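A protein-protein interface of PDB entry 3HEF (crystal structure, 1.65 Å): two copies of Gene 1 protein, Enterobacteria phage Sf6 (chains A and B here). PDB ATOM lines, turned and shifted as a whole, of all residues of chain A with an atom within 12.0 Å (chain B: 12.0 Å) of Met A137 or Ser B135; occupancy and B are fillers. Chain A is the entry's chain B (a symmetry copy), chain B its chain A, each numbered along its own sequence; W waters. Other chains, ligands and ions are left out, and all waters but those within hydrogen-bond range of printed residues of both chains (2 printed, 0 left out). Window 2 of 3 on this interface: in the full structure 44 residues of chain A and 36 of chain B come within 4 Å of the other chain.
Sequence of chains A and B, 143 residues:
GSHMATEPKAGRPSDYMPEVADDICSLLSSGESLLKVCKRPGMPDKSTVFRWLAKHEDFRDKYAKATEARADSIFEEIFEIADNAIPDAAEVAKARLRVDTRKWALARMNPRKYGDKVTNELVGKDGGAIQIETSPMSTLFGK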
ATOM      1  N   GLU A 133     -29.368 -29.133   7.055  1.00  0.00           N
ATOM      2  CA  GLU A 133     -29.622 -29.477   5.652  1.00  0.00           C
ATOM      3  C   GLU A 133     -28.270 -29.646   4.980  1.00  0.00           C
ATOM      4  O   GLU A 133     -27.449 -28.719   4.973  1.00  0.00           O
ATOM      5  CB  GLU A 133     -30.313 -28.349   4.915  1.00  0.00           C
ATOM      6  CG  GLU A 133     -31.804 -28.362   4.874  1.00  0.00           C
ATOM      7  CD  GLU A 133     -32.294 -27.330   3.884  1.00  0.00           C
ATOM      8  OE1 GLU A 133     -31.903 -27.421   2.701  1.00  0.00           O
ATOM      9  OE2 GLU A 133     -33.056 -26.433   4.288  1.00  0.00           O
ATOM     10  N   THR A 134     -28.035 -30.818   4.400  1.00  0.00           N
ATOM     11  CA  THR A 134     -26.771 -31.066   3.724  1.00  0.00           C
ATOM     12  C   THR A 134     -27.019 -30.951   2.223  1.00  0.00           C
ATOM     13  O   THR A 134     -28.097 -31.285   1.738  1.00  0.00           O
ATOM     14  CB  THR A 134     -26.242 -32.465   4.034  1.00  0.00           C
ATOM     15  OG1 THR A 134     -27.251 -33.426   3.702  1.00  0.00           O
ATOM     16  CG2 THR A 134     -25.882 -32.589   5.518  1.00  0.00           C
ATOM     17  N   SER A 135     -26.021 -30.469   1.499  1.00  0.00           N
ATOM     18  CA  SER A 135     -26.140 -30.279   0.061  1.00  0.00           C
ATOM     19  C   SER A 135     -24.816 -30.597  -0.585  1.00  0.00           C
ATOM     20  O   SER A 135     -23.775 -30.621   0.081  1.00  0.00           O
ATOM     21  CB  SER A 135     -26.496 -28.832  -0.252  1.00  0.00           C
ATOM     22  OG  SER A 135     -27.717 -28.464   0.358  1.00  0.00           O
ATOM     23  N   PRO A 136     -24.837 -30.880  -1.902  1.00  0.00           N
ATOM     24  CA  PRO A 136     -23.593 -31.194  -2.612  1.00  0.00           C
ATOM     25  C   PRO A 136     -22.771 -29.906  -2.655  1.00  0.00           C
ATOM     26  O   PRO A 136     -23.329 -28.802  -2.669  1.00  0.00           O
ATOM     27  CB  PRO A 136     -24.081 -31.608  -4.003  1.00  0.00           C
ATOM     28  CG  PRO A 136     -25.507 -32.095  -3.749  1.00  0.00           C
ATOM     29  CD  PRO A 136     -26.007 -31.058  -2.779  1.00  0.00           C
ATOM     30  N   MET A 137     -21.454 -30.041  -2.686  1.00  0.00           N
ATOM     31  CA  MET A 137     -20.620 -28.863  -2.725  1.00  0.00           C
ATOM     32  C   MET A 137     -20.970 -28.043  -3.958  1.00  0.00           C
ATOM     33  O   MET A 137     -21.209 -28.587  -5.041  1.00  0.00           O
ATOM     34  CB  MET A 137     -19.143 -29.261  -2.702  1.00  0.00           C
ATOM     35  CG  MET A 137     -18.676 -30.112  -3.843  1.00  0.00           C
ATOM     36  SD  MET A 137     -17.142 -30.906  -3.332  1.00  0.00           S
ATOM     37  CE  MET A 137     -15.988 -29.489  -3.274  1.00  0.00           C
ATOM     38  N   SER A 138     -21.045 -26.732  -3.777  1.00  0.00           N
ATOM     39  CA  SER A 138     -21.373 -25.826  -4.861  1.00  0.00           C
ATOM     40  C   SER A 138     -20.127 -25.108  -5.380  1.00  0.00           C
ATOM     41  O   SER A 138     -20.191 -24.410  -6.389  1.00  0.00           O
ATOM     42  CB  SER A 138     -22.405 -24.806  -4.391  1.00  0.00           C
ATOM     43  OG  SER A 138     -21.883 -24.068  -3.310  1.00  0.00           O
ATOM     44  N   THR A 139     -19.005 -25.255  -4.675  1.00  0.00           N
ATOM     45  CA  THR A 139     -17.734 -24.644  -5.088  1.00  0.00           C
ATOM     46  C   THR A 139     -16.592 -25.620  -4.847  1.00  0.00           C
ATOM     47  O   THR A 139     -16.723 -26.549  -4.051  1.00  0.00           O
ATOM     48  CB  THR A 139     -17.414 -23.354  -4.307  1.00  0.00           C
ATOM     49  OG1 THR A 139     -17.153 -23.682  -2.936  1.00  0.00           O
ATOM     50  CG2 THR A 139     -18.565 -22.375  -4.391  1.00  0.00           C
ATOM     51  N   LEU A 140     -15.465 -25.404  -5.524  1.00  0.00           N
ATOM     52  CA  LEU A 140     -14.300 -26.274  -5.386  1.00  0.00           C
ATOM     53  C   LEU A 140     -13.495 -25.962  -4.136  1.00  0.00           C
ATOM     54  O   LEU A 140     -12.426 -25.339  -4.221  1.00  0.00           O
ATOM     55  CB  LEU A 140     -13.387 -26.133  -6.609  1.00  0.00           C
ATOM     56  CG  LEU A 140     -13.756 -26.928  -7.851  1.00  0.00           C
ATOM     57  CD1 LEU A 140     -13.081 -26.327  -9.101  1.00  0.00           C
ATOM     58  CD2 LEU A 140     -13.314 -28.365  -7.634  1.00  0.00           C
ATOM     59  N   PHE A 141     -13.975 -26.417  -2.982  1.00  0.00           N
ATOM     60  CA  PHE A 141     -13.266 -26.140  -1.734  1.00  0.00           C
ATOM     61  C   PHE A 141     -12.405 -27.282  -1.187  1.00  0.00           C
ATOM     62  O   PHE A 141     -11.811 -27.153  -0.112  1.00  0.00           O
ATOM     63  CB  PHE A 141     -14.257 -25.675  -0.661  1.00  0.00           C
ATOM     64  CG  PHE A 141     -15.313 -26.687  -0.296  1.00  0.00           C
ATOM     65  CD1 PHE A 141     -14.996 -27.822   0.452  1.00  0.00           C
ATOM     66  CD2 PHE A 141     -16.650 -26.434  -0.582  1.00  0.00           C
ATOM     67  CE1 PHE A 141     -15.994 -28.670   0.923  1.00  0.00           C
ATOM     68  CE2 PHE A 141     -17.653 -27.278  -0.115  1.00  0.00           C
ATOM     69  CZ  PHE A 141     -17.330 -28.386   0.637  1.00  0.00           C
ATOM     70  N   GLY A 142     -12.331 -28.386  -1.928  1.00  0.00           N
ATOM     71  CA  GLY A 142     -11.535 -29.528  -1.495  1.00  0.00           C
ATOM     72  C   GLY A 142     -10.030 -29.354  -1.648  1.00  0.00           C
ATOM     73  O   GLY A 142      -9.571 -28.243  -2.012  1.00  0.00           O
ATOM     74  N   GLN B 131     -27.023 -24.787   6.965  1.00  0.00           N
ATOM     75  CA  GLN B 131     -26.612 -25.304   5.648  1.00  0.00           C
ATOM     76  C   GLN B 131     -25.183 -25.839   5.658  1.00  0.00           C
ATOM     77  O   GLN B 131     -24.230 -25.117   5.951  1.00  0.00           O
ATOM     78  CB  GLN B 131     -26.746 -24.189   4.597  1.00  0.00           C
ATOM     79  CG  GLN B 131     -28.161 -23.612   4.474  1.00  0.00           C
ATOM     80  CD  GLN B 131     -29.184 -24.641   4.086  1.00  0.00           C
ATOM     81  OE1 GLN B 131     -30.244 -24.741   4.698  1.00  0.00           O
ATOM     82  NE2 GLN B 131     -28.878 -25.410   3.049  1.00  0.00           N
ATOM     83  N   ILE B 132     -25.008 -27.109   5.282  1.00  0.00           N
ATOM     84  CA  ILE B 132     -23.674 -27.690   5.272  1.00  0.00           C
ATOM     85  C   ILE B 132     -23.450 -28.343   3.904  1.00  0.00           C
ATOM     86  O   ILE B 132     -24.370 -28.939   3.373  1.00  0.00           O
ATOM     87  CB  ILE B 132     -23.566 -28.785   6.331  1.00  0.00           C
ATOM     88  CG1 ILE B 132     -23.668 -28.156   7.736  1.00  0.00           C
ATOM     89  CG2 ILE B 132     -22.262 -29.536   6.198  1.00  0.00           C
ATOM     90  CD1 ILE B 132     -23.699 -29.175   8.859  1.00  0.00           C
ATOM     91  N   GLU B 133     -22.252 -28.167   3.360  1.00  0.00           N
ATOM     92  CA  GLU B 133     -21.849 -28.820   2.108  1.00  0.00           C
ATOM     93  C   GLU B 133     -20.655 -29.695   2.483  1.00  0.00           C
ATOM     94  O   GLU B 133     -19.734 -29.250   3.183  1.00  0.00           O
ATOM     95  CB  GLU B 133     -21.397 -27.803   1.054  1.00  0.00           C
ATOM     96  CG  GLU B 133     -22.534 -27.135   0.344  1.00  0.00           C
ATOM     97  CD  GLU B 133     -22.090 -26.020  -0.587  1.00  0.00           C
ATOM     98  OE1 GLU B 133     -20.902 -26.006  -1.005  1.00  0.00           O
ATOM     99  OE2 GLU B 133     -22.947 -25.167  -0.913  1.00  0.00           O
ATOM    100  N   THR B 134     -20.636 -30.941   2.032  1.00  0.00           N
ATOM    101  CA  THR B 134     -19.483 -31.764   2.366  1.00  0.00           C
ATOM    102  C   THR B 134     -18.713 -32.273   1.138  1.00  0.00           C
ATOM    103  O   THR B 134     -19.280 -32.415   0.055  1.00  0.00           O
ATOM    104  CB  THR B 134     -19.891 -32.959   3.238  1.00  0.00           C
ATOM    105  OG1 THR B 134     -20.546 -32.481   4.426  1.00  0.00           O
ATOM    106  CG2 THR B 134     -18.657 -33.738   3.665  1.00  0.00           C
ATOM    107  N   SER B 135     -17.412 -32.493   1.324  1.00  0.00           N
ATOM    108  CA  SER B 135     -16.510 -33.011   0.291  1.00  0.00           C
ATOM    109  C   SER B 135     -15.837 -34.246   0.873  1.00  0.00           C
ATOM    110  O   SER B 135     -15.157 -34.087   1.911  1.00  0.00           O
ATOM    111  CB  SER B 135     -15.408 -32.009  -0.051  1.00  0.00           C
ATOM    112  OG  SER B 135     -15.915 -30.875  -0.723  1.00  0.00           O
HETATM  113  O   HOH W   1     -19.453 -23.732  -1.139  1.00  0.00           O
HETATM  114  O   HOH W   2     -26.909 -27.095   2.318  1.00  0.00           O
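Of the 5 printed residues of chain B, 5 touch a printed residue of chain A.
Of the 10 printed residues of chain A, 7 touch a printed residue of chain B.
Hydrophobic or aromatic side chains of chain A within 4 Å of the printed part of chain B: Met A137 and Phe A141.
Among the printed residues, 12 pairs touch across the chains.
Among the printed residues, no Asp or Glu carboxylate lies within 4 Å of a Lys or Arg side-chain nitrogen of the other chain.
O of Ile B132 touches CA of Thr A134 (3.2 Å).
Glu B133 touches Ser A135.
Thr B134 touches Ser A135.
Glu B133 touches Pro A136 (CG to O, 3.5 Å).
Glu B133 touches Met A137.
Glu B133 touches Phe A141.
Phe A141 touches Ser B135.
The side-chain hydroxyl (OG) of Ser A138 sits at hydrogen-bond distance from the side-chain carboxylate (OE2) of Glu B133 (2.8 Å).
O of Ile B132 is in hydrogen-bond range of N of Ser A135, 2.9 Å away.
The side-chain carboxylate (OE2) of Glu A133 lies close to the side-chain amide oxygen (OE1) of Gln B131, at 3.3 Å.
OG of Ser B135 lies within hydrogen-bond range of SD of Met A137 (2.9 Å).
The backbone carbonyl oxygen (O) of Glu A133 is in hydrogen-bond range of the backbone NH (N) of Ile B132, 2.9 Å away.
Of chain B, only Glu B133 (3.5 Å) comes within 4 Å of Pro A136.
Leu A140 touches none of the printed residues of chain B.
Phe A141 touches two residues of chain B.
No residue of chain B comes within 4 Å of Gly A142.
Of the printed residues of chain A, Gln B131 touches Glu A133 (3.3 Å).
Of the printed residues of chain A, Ile B132 touches Glu A133, Thr A134 and Ser A135.
Of chain A, only Ser A135, Pro A136, Met A137, Ser A138 and Phe A141 come within 4 Å of Glu B133.
Thr B134 touches one residue of chain A.
Ser B135 touches two residues of chain A.
The nearest residue of chain B that does not touch Met A137 is Thr B134 (4.2 Å).
The nearest residue of chain A that does not touch Ser B135 is Gly A142 (4.5 Å).
The nearest printed residue of chain A that does not touch Gln B131 is Ser A135 (4.2 Å).
Ser A135 touches Glu B133, but with the chains exchanged Glu A133 does not touch Ser B135 (11.3 Å).
Ser A135 touches Thr B134, but with the chains exchanged Thr A134 does not touch Ser B135 (9.2 Å).
Positions printed for both chains: 133, 134 and 135.
Water W2 lies within hydrogen-bond range of the side-chain hydroxyl of Ser A135, the side-chain amide nitrogen of Gln B131, the backbone carbonyl oxygen of Glu A133 and the backbone carbonyl oxygen of Ile B132.
Water W1 lies within hydrogen-bond range of OE1 of Glu B133, OG1 of Thr A139 and OG of Ser A138.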
